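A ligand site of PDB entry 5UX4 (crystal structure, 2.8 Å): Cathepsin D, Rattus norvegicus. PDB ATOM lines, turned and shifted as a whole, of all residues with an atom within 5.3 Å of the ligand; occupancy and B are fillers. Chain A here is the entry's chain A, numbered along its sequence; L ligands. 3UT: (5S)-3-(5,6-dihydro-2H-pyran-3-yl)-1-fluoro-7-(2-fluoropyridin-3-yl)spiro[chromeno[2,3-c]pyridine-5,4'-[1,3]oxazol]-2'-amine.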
ATOM      1  N   ALA A  76      15.799  31.030  21.475  1.00  0.00           N
ATOM      2  CA  ALA A  76      15.860  30.108  20.354  1.00  0.00           C
ATOM      3  C   ALA A  76      15.234  30.651  19.079  1.00  0.00           C
ATOM      4  O   ALA A  76      15.703  30.308  17.992  1.00  0.00           O
ATOM      5  CB  ALA A  76      15.178  28.785  20.713  1.00  0.00           C
ATOM      6  N   GLN A  77      14.193  31.468  19.184  1.00  0.00           N
ATOM      7  CA  GLN A  77      13.500  32.001  18.028  1.00  0.00           C
ATOM      8  C   GLN A  77      13.440  33.519  18.108  1.00  0.00           C
ATOM      9  O   GLN A  77      13.126  34.081  19.157  1.00  0.00           O
ATOM     10  CB  GLN A  77      12.086  31.430  17.918  1.00  0.00           C
ATOM     11  CG  GLN A  77      12.049  29.923  17.746  1.00  0.00           C
ATOM     12  CD  GLN A  77      10.634  29.371  17.733  1.00  0.00           C
ATOM     13  OE1 GLN A  77       9.711  30.008  17.233  1.00  0.00           O
ATOM     14  NE2 GLN A  77      10.464  28.181  18.291  1.00  0.00           N
ATOM     15  N   VAL A  94      10.632  34.775  10.706  1.00  0.00           N
ATOM     16  CA  VAL A  94      12.041  34.793  11.075  1.00  0.00           C
ATOM     17  C   VAL A  94      12.812  35.364   9.883  1.00  0.00           C
ATOM     18  O   VAL A  94      12.737  34.829   8.778  1.00  0.00           O
ATOM     19  CB  VAL A  94      12.558  33.392  11.435  1.00  0.00           C
ATOM     20  CG1 VAL A  94      14.079  33.353  11.383  1.00  0.00           C
ATOM     21  CG2 VAL A  94      12.065  33.001  12.821  1.00  0.00           C
ATOM     22  N   ASP A  96      15.657  35.312   8.032  1.00  0.00           N
ATOM     23  CA  ASP A  96      16.620  34.232   7.996  1.00  0.00           C
ATOM     24  C   ASP A  96      17.681  34.518   6.940  1.00  0.00           C
ATOM     25  O   ASP A  96      17.386  34.536   5.734  1.00  0.00           O
ATOM     26  CB  ASP A  96      15.912  32.914   7.718  1.00  0.00           C
ATOM     27  CG  ASP A  96      16.857  31.742   7.609  1.00  0.00           C
ATOM     28  OD1 ASP A  96      17.978  31.816   8.159  1.00  0.00           O
ATOM     29  OD2 ASP A  96      16.470  30.744   6.962  1.00  0.00           O
ATOM     30  N   GLY A  98      19.912  32.403   6.353  1.00  0.00           N
ATOM     31  CA  GLY A  98      20.259  31.076   5.884  1.00  0.00           C
ATOM     32  C   GLY A  98      19.398  30.550   4.761  1.00  0.00           C
ATOM     33  O   GLY A  98      19.584  29.408   4.341  1.00  0.00           O
ATOM     34  N   SER A  99      18.454  31.348   4.267  1.00  0.00           N
ATOM     35  CA  SER A  99      17.671  31.018   3.090  1.00  0.00           C
ATOM     36  C   SER A  99      17.409  32.307   2.309  1.00  0.00           C
ATOM     37  O   SER A  99      17.915  33.376   2.667  1.00  0.00           O
ATOM     38  CB  SER A  99      16.362  30.305   3.464  1.00  0.00           C
ATOM     39  OG  SER A  99      15.506  31.150   4.207  1.00  0.00           O
ATOM     40  N   ASN A 101      14.002  32.721   0.459  1.00  0.00           N
ATOM     41  CA  ASN A 101      12.616  32.761   0.042  1.00  0.00           C
ATOM     42  C   ASN A 101      11.734  33.339   1.143  1.00  0.00           C
ATOM     43  O   ASN A 101      12.049  33.223   2.337  1.00  0.00           O
ATOM     44  CB  ASN A 101      12.101  31.371  -0.340  1.00  0.00           C
ATOM     45  CG  ASN A 101      12.794  30.816  -1.574  1.00  0.00           C
ATOM     46  OD1 ASN A 101      13.691  29.982  -1.471  1.00  0.00           O
ATOM     47  ND2 ASN A 101      12.380  31.284  -2.749  1.00  0.00           N
ATOM     48  N   TRP A 103       7.900  32.919   2.519  1.00  0.00           N
ATOM     49  CA  TRP A 103       6.704  32.101   2.449  1.00  0.00           C
ATOM     50  C   TRP A 103       5.942  32.184   3.765  1.00  0.00           C
ATOM     51  O   TRP A 103       6.532  32.332   4.832  1.00  0.00           O
ATOM     52  CB  TRP A 103       7.016  30.644   2.102  1.00  0.00           C
ATOM     53  CG  TRP A 103       7.927  29.949   3.071  1.00  0.00           C
ATOM     54  CD1 TRP A 103       9.279  29.760   2.927  1.00  0.00           C
ATOM     55  CD2 TRP A 103       7.570  29.327   4.313  1.00  0.00           C
ATOM     56  NE1 TRP A 103       9.772  29.077   4.012  1.00  0.00           N
ATOM     57  CE2 TRP A 103       8.743  28.800   4.876  1.00  0.00           C
ATOM     58  CE3 TRP A 103       6.366  29.179   5.008  1.00  0.00           C
ATOM     59  CZ2 TRP A 103       8.755  28.124   6.094  1.00  0.00           C
ATOM     60  CZ3 TRP A 103       6.366  28.512   6.217  1.00  0.00           C
ATOM     61  CH2 TRP A 103       7.559  27.996   6.753  1.00  0.00           C
ATOM     62  N   ILE A 139      10.081  22.871  -1.251  1.00  0.00           N
ATOM     63  CA  ILE A 139      11.281  23.269  -0.540  1.00  0.00           C
ATOM     64  C   ILE A 139      11.667  22.169   0.443  1.00  0.00           C
ATOM     65  O   ILE A 139      10.816  21.689   1.213  1.00  0.00           O
ATOM     66  CB  ILE A 139      11.087  24.609   0.193  1.00  0.00           C
ATOM     67  CG1 ILE A 139      10.812  25.730  -0.823  1.00  0.00           C
ATOM     68  CG2 ILE A 139      12.299  24.948   1.034  1.00  0.00           C
ATOM     69  CD1 ILE A 139      10.620  27.095  -0.197  1.00  0.00           C
ATOM     70  N   HIS A 140      12.937  21.777   0.424  1.00  0.00           N
ATOM     71  CA  HIS A 140      13.468  20.749   1.315  1.00  0.00           C
ATOM     72  C   HIS A 140      14.655  21.294   2.101  1.00  0.00           C
ATOM     73  O   HIS A 140      15.391  22.166   1.617  1.00  0.00           O
ATOM     74  CB  HIS A 140      13.914  19.507   0.519  1.00  0.00           C
ATOM     75  CG  HIS A 140      12.786  18.744  -0.091  1.00  0.00           C
ATOM     76  ND1 HIS A 140      12.114  17.738   0.579  1.00  0.00           N
ATOM     77  CD2 HIS A 140      12.214  18.824  -1.310  1.00  0.00           C
ATOM     78  CE1 HIS A 140      11.181  17.246  -0.209  1.00  0.00           C
ATOM     79  NE2 HIS A 140      11.212  17.886  -1.362  1.00  0.00           N
ATOM     80  N   TYR A 141      14.835  20.760   3.306  1.00  0.00           N
ATOM     81  CA  TYR A 141      15.993  21.071   4.128  1.00  0.00           C
ATOM     82  C   TYR A 141      16.101  19.995   5.213  1.00  0.00           C
ATOM     83  O   TYR A 141      15.414  18.965   5.157  1.00  0.00           O
ATOM     84  CB  TYR A 141      15.918  22.482   4.707  1.00  0.00           C
ATOM     85  CG  TYR A 141      14.957  22.654   5.864  1.00  0.00           C
ATOM     86  CD1 TYR A 141      13.584  22.647   5.663  1.00  0.00           C
ATOM     87  CD2 TYR A 141      15.432  22.842   7.154  1.00  0.00           C
ATOM     88  CE1 TYR A 141      12.716  22.800   6.715  1.00  0.00           C
ATOM     89  CE2 TYR A 141      14.571  23.006   8.209  1.00  0.00           C
ATOM     90  CZ  TYR A 141      13.213  22.984   7.994  1.00  0.00           C
ATOM     91  OH  TYR A 141      12.344  23.137   9.046  1.00  0.00           O
ATOM     92  N   LEU A 146       8.338  21.625   2.943  1.00  0.00           N
ATOM     93  CA  LEU A 146       7.032  22.242   2.727  1.00  0.00           C
ATOM     94  C   LEU A 146       6.848  22.476   1.235  1.00  0.00           C
ATOM     95  O   LEU A 146       7.814  22.454   0.474  1.00  0.00           O
ATOM     96  CB  LEU A 146       6.879  23.559   3.507  1.00  0.00           C
ATOM     97  CG  LEU A 146       7.727  24.741   3.048  1.00  0.00           C
ATOM     98  CD1 LEU A 146       6.993  26.042   3.285  1.00  0.00           C
ATOM     99  CD2 LEU A 146       9.073  24.750   3.762  1.00  0.00           C
ATOM    100  N   VAL A 183       8.006  19.952  12.736  1.00  0.00           N
ATOM    101  CA  VAL A 183       8.864  21.116  12.910  1.00  0.00           C
ATOM    102  C   VAL A 183       8.028  22.361  13.162  1.00  0.00           C
ATOM    103  O   VAL A 183       8.172  23.043  14.190  1.00  0.00           O
ATOM    104  CB  VAL A 183       9.782  21.306  11.683  1.00  0.00           C
ATOM    105  CG1 VAL A 183      10.914  22.261  12.010  1.00  0.00           C
ATOM    106  CG2 VAL A 183      10.308  19.956  11.202  1.00  0.00           C
ATOM    107  N   PHE A 184       7.134  22.687  12.219  1.00  0.00           N
ATOM    108  CA  PHE A 184       6.413  23.946  12.241  1.00  0.00           C
ATOM    109  C   PHE A 184       5.414  24.052  13.382  1.00  0.00           C
ATOM    110  O   PHE A 184       4.903  25.145  13.627  1.00  0.00           O
ATOM    111  CB  PHE A 184       5.715  24.142  10.903  1.00  0.00           C
ATOM    112  CG  PHE A 184       6.656  24.188   9.735  1.00  0.00           C
ATOM    113  CD1 PHE A 184       7.746  25.049   9.751  1.00  0.00           C
ATOM    114  CD2 PHE A 184       6.483  23.358   8.640  1.00  0.00           C
ATOM    115  CE1 PHE A 184       8.630  25.091   8.683  1.00  0.00           C
ATOM    116  CE2 PHE A 184       7.359  23.389   7.570  1.00  0.00           C
ATOM    117  CZ  PHE A 184       8.435  24.265   7.599  1.00  0.00           C
ATOM    118  N   PHE A 189       6.454  31.297  15.081  1.00  0.00           N
ATOM    119  CA  PHE A 189       6.366  32.226  13.972  1.00  0.00           C
ATOM    120  C   PHE A 189       5.653  31.587  12.795  1.00  0.00           C
ATOM    121  O   PHE A 189       5.683  30.366  12.620  1.00  0.00           O
ATOM    122  CB  PHE A 189       7.766  32.701  13.534  1.00  0.00           C
ATOM    123  CG  PHE A 189       8.733  31.582  13.263  1.00  0.00           C
ATOM    124  CD1 PHE A 189       8.834  31.037  11.996  1.00  0.00           C
ATOM    125  CD2 PHE A 189       9.533  31.072  14.284  1.00  0.00           C
ATOM    126  CE1 PHE A 189       9.723  30.002  11.743  1.00  0.00           C
ATOM    127  CE2 PHE A 189      10.410  30.044  14.032  1.00  0.00           C
ATOM    128  CZ  PHE A 189      10.510  29.509  12.767  1.00  0.00           C
ATOM    129  N   ILE A 192       8.930  32.422   7.043  1.00  0.00           N
ATOM    130  CA  ILE A 192      10.346  32.758   6.901  1.00  0.00           C
ATOM    131  C   ILE A 192      10.497  33.814   5.819  1.00  0.00           C
ATOM    132  O   ILE A 192       9.839  33.741   4.777  1.00  0.00           O
ATOM    133  CB  ILE A 192      11.181  31.503   6.554  1.00  0.00           C
ATOM    134  CG1 ILE A 192      11.129  30.496   7.692  1.00  0.00           C
ATOM    135  CG2 ILE A 192      12.630  31.886   6.240  1.00  0.00           C
ATOM    136  CD1 ILE A 192      11.854  29.228   7.349  1.00  0.00           C
ATOM    137  N   ILE A 200      20.723  30.826  -3.764  1.00  0.00           N
ATOM    138  CA  ILE A 200      20.083  29.700  -3.091  1.00  0.00           C
ATOM    139  C   ILE A 200      18.575  29.872  -3.007  1.00  0.00           C
ATOM    140  O   ILE A 200      17.916  29.189  -2.229  1.00  0.00           O
ATOM    141  CB  ILE A 200      20.692  29.471  -1.690  1.00  0.00           C
ATOM    142  CG1 ILE A 200      20.542  30.741  -0.839  1.00  0.00           C
ATOM    143  CG2 ILE A 200      22.148  29.045  -1.805  1.00  0.00           C
ATOM    144  CD1 ILE A 200      20.719  30.498   0.640  1.00  0.00           C
ATOM    145  N   VAL A 202      15.072  29.088  -4.021  1.00  0.00           N
ATOM    146  CA  VAL A 202      14.361  28.052  -4.747  1.00  0.00           C
ATOM    147  C   VAL A 202      13.377  28.699  -5.709  1.00  0.00           C
ATOM    148  O   VAL A 202      12.643  29.634  -5.342  1.00  0.00           O
ATOM    149  CB  VAL A 202      13.658  27.094  -3.769  1.00  0.00           C
ATOM    150  CG1 VAL A 202      12.814  26.078  -4.524  1.00  0.00           C
ATOM    151  CG2 VAL A 202      14.680  26.390  -2.891  1.00  0.00           C
ATOM    152  N   TYR A 263      25.073  31.409   0.823  1.00  0.00           N
ATOM    153  CA  TYR A 263      24.857  31.823   2.190  1.00  0.00           C
ATOM    154  C   TYR A 263      25.763  33.009   2.493  1.00  0.00           C
ATOM    155  O   TYR A 263      26.566  33.441   1.660  1.00  0.00           O
ATOM    156  CB  TYR A 263      25.140  30.674   3.159  1.00  0.00           C
ATOM    157  CG  TYR A 263      24.349  29.407   2.901  1.00  0.00           C
ATOM    158  CD1 TYR A 263      23.003  29.340   3.210  1.00  0.00           C
ATOM    159  CD2 TYR A 263      24.958  28.288   2.354  1.00  0.00           C
ATOM    160  CE1 TYR A 263      22.270  28.184   2.980  1.00  0.00           C
ATOM    161  CE2 TYR A 263      24.247  27.127   2.122  1.00  0.00           C
ATOM    162  CZ  TYR A 263      22.905  27.090   2.439  1.00  0.00           C
ATOM    163  OH  TYR A 263      22.182  25.936   2.209  1.00  0.00           O
ATOM    164  N   ASP A 289      24.314  32.758  10.250  1.00  0.00           N
ATOM    165  CA  ASP A 289      22.941  32.341  10.013  1.00  0.00           C
ATOM    166  C   ASP A 289      22.066  32.745  11.197  1.00  0.00           C
ATOM    167  O   ASP A 289      22.180  32.173  12.277  1.00  0.00           O
ATOM    168  CB  ASP A 289      22.867  30.826   9.797  1.00  0.00           C
ATOM    169  CG  ASP A 289      21.473  30.352   9.423  1.00  0.00           C
ATOM    170  OD1 ASP A 289      21.289  29.121   9.282  1.00  0.00           O
ATOM    171  OD2 ASP A 289      20.571  31.189   9.249  1.00  0.00           O
ATOM    172  N   THR A 290      21.181  33.723  10.974  1.00  0.00           N
ATOM    173  CA  THR A 290      20.218  34.116  11.988  1.00  0.00           C
ATOM    174  C   THR A 290      19.072  33.115  12.123  1.00  0.00           C
ATOM    175  O   THR A 290      18.290  33.226  13.074  1.00  0.00           O
ATOM    176  CB  THR A 290      19.641  35.496  11.662  1.00  0.00           C
ATOM    177  OG1 THR A 290      18.984  35.457  10.382  1.00  0.00           O
ATOM    178  CG2 THR A 290      20.739  36.550  11.620  1.00  0.00           C
ATOM    179  N   GLY A 291      18.951  32.159  11.215  1.00  0.00           N
ATOM    180  CA  GLY A 291      17.877  31.192  11.267  1.00  0.00           C
ATOM    181  C   GLY A 291      18.261  29.892  11.936  1.00  0.00           C
ATOM    182  O   GLY A 291      17.615  28.864  11.727  1.00  0.00           O
ATOM    183  N   THR A 292      19.333  29.921  12.720  1.00  0.00           N
ATOM    184  CA  THR A 292      19.794  28.774  13.479  1.00  0.00           C
ATOM    185  C   THR A 292      19.999  29.193  14.929  1.00  0.00           C
ATOM    186  O   THR A 292      20.654  30.211  15.187  1.00  0.00           O
ATOM    187  CB  THR A 292      21.096  28.202  12.904  1.00  0.00           C
ATOM    188  OG1 THR A 292      20.990  28.111  11.482  1.00  0.00           O
ATOM    189  CG2 THR A 292      21.363  26.808  13.465  1.00  0.00           C
ATOM    190  N   SER A 293      19.426  28.431  15.855  1.00  0.00           N
ATOM    191  CA  SER A 293      19.477  28.817  17.263  1.00  0.00           C
ATOM    192  C   SER A 293      20.894  28.732  17.814  1.00  0.00           C
ATOM    193  O   SER A 293      21.393  29.689  18.423  1.00  0.00           O
ATOM    194  CB  SER A 293      18.537  27.932  18.078  1.00  0.00           C
ATOM    195  OG  SER A 293      17.200  28.009  17.590  1.00  0.00           O
ATOM    196  N   ASP A 381      22.342  32.055  16.375  1.00  0.00           N
ATOM    197  CA  ASP A 381      21.862  33.126  17.243  1.00  0.00           C
ATOM    198  C   ASP A 381      22.712  33.285  18.495  1.00  0.00           C
ATOM    199  O   ASP A 381      22.760  34.376  19.073  1.00  0.00           O
ATOM    200  CB  ASP A 381      20.404  32.874  17.619  1.00  0.00           C
ATOM    201  CG  ASP A 381      19.480  32.868  16.412  1.00  0.00           C
ATOM    202  OD1 ASP A 381      19.748  33.635  15.460  1.00  0.00           O
ATOM    203  OD2 ASP A 381      18.494  32.099  16.411  1.00  0.00           O
HETATM  204  C28 3UT L   1      17.692  26.448   2.997  1.00  0.00           C
HETATM  205  O29 3UT L   1      18.371  26.298   1.581  1.00  0.00           O
HETATM  206  C30 3UT L   1      17.667  26.860   0.647  1.00  0.00           C
HETATM  207  C31 3UT L   1      16.154  26.247   0.453  1.00  0.00           C
HETATM  208  C32 3UT L   1      15.512  26.169   1.662  1.00  0.00           C
HETATM  209  C20 3UT L   1      16.244  26.570   2.937  1.00  0.00           C
HETATM  210  C13 3UT L   1      15.437  26.478   4.200  1.00  0.00           C
HETATM  211  C14 3UT L   1      15.985  26.787   5.439  1.00  0.00           C
HETATM  212  N12 3UT L   1      14.182  26.102   4.069  1.00  0.00           N
HETATM  213  C11 3UT L   1      13.365  25.988   5.100  1.00  0.00           C
HETATM  214  F33 3UT L   1      12.042  25.585   4.981  1.00  0.00           F
HETATM  215  C8  3UT L   1      13.868  26.294   6.399  1.00  0.00           C
HETATM  216  O7  3UT L   1      12.904  26.143   7.459  1.00  0.00           O
HETATM  217  C9  3UT L   1      15.176  26.699   6.589  1.00  0.00           C
HETATM  218  C10 3UT L   1      15.713  27.047   8.011  1.00  0.00           C
HETATM  219  C15 3UT L   1      16.691  25.944   8.403  1.00  0.00           C
HETATM  220  O16 3UT L   1      17.997  26.512   8.611  1.00  0.00           O
HETATM  221  C17 3UT L   1      17.862  27.952   8.373  1.00  0.00           C
HETATM  222  N18 3UT L   1      16.443  28.190   8.023  1.00  0.00           N
HETATM  223  N19 3UT L   1      18.894  28.986   8.448  1.00  0.00           N
HETATM  224  C5  3UT L   1      14.621  27.052   9.002  1.00  0.00           C
HETATM  225  C6  3UT L   1      14.963  27.523  10.263  1.00  0.00           C
HETATM  226  C4  3UT L   1      13.331  26.635   8.747  1.00  0.00           C
HETATM  227  C3  3UT L   1      12.323  26.693   9.722  1.00  0.00           C
HETATM  228  C2  3UT L   1      12.677  27.160  10.962  1.00  0.00           C
HETATM  229  C1  3UT L   1      13.966  27.571  11.246  1.00  0.00           C
HETATM  230  C21 3UT L   1      14.188  28.021  12.530  1.00  0.00           C
HETATM  231  C26 3UT L   1      13.849  27.168  13.564  1.00  0.00           C
HETATM  232  C25 3UT L   1      14.023  27.597  14.852  1.00  0.00           C
HETATM  233  C24 3UT L   1      14.521  28.869  15.052  1.00  0.00           C
HETATM  234  N23 3UT L   1      14.818  29.665  14.045  1.00  0.00           N
HETATM  235  C22 3UT L   1      14.663  29.283  12.799  1.00  0.00           C
HETATM  236  F27 3UT L   1      14.992  30.132  11.775  1.00  0.00           F
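A nitrogen (N19) of the ligand is in hydrogen-bond range of the side-chain carboxylate (OD1) of Asp 289, 2.5 Å away.
The side-chain carboxylate (OD2) of Asp 96 sits at hydrogen-bond distance from a nitrogen (N18) of the ligand, at 2.8 Å.
An oxygen (O7) of the ligand sits close to the side-chain hydroxyl of Tyr 141, 3.4 Å away.
OD2 of Asp 289 is in hydrogen-bond range of N of Gly 291 (2.7 Å).
The side-chain carboxylate of Asp 96 sits close to the backbone NH of Gly 291 (3.2 Å).
The side-chain carboxylate of Asp 96 is in hydrogen-bond range of the backbone NH of Gly 98, at 2.7 Å.
OG of Ser 99 is in hydrogen-bond range of OD2 of Asp 96 (2.9 Å).
O of Leu 146 is in hydrogen-bond range of N of Ile 139 (2.9 Å).
The backbone carbonyl oxygen (O) of Ala 76 lies within hydrogen-bond range of the side-chain hydroxyl (OG) of Ser 293, at 2.8 Å.
The backbone NH (N) of Asp 381 lies within hydrogen-bond range of the backbone carbonyl oxygen (O) of Ser 293, at 3.3 Å.
The backbone carbonyl oxygen (O) of Thr 292 sits at hydrogen-bond distance from the backbone NH (N) of Asp 381, at 2.8 Å.
F27 of the ligand lies close to O of Gly 291.
Residues that only touch the ligand: Ile 192 (3.3 Å), Leu 146 (3.3 Å), Val 94 (3.4 Å), Ala 76 (3.5 Å), Ile 139 (3.5 Å), Gly 98 (3.6 Å), Val 202 (3.7 Å), Phe 189 (3.7 Å), Ile 200 (3.7 Å), Ser 99 (3.8 Å), Ser 293 (3.8 Å), Thr 292 (3.8 Å), Gln 77 (3.8 Å) and Tyr 263 (3.9 Å).
Hydrophobic or aromatic side chains within 4 Å of the ligand: Val 94, Ile 139, Tyr 141, Leu 146, Phe 189, Ile 192 and Val 202.
Of the 25 residues printed, 18 come within 4 Å of the ligand.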
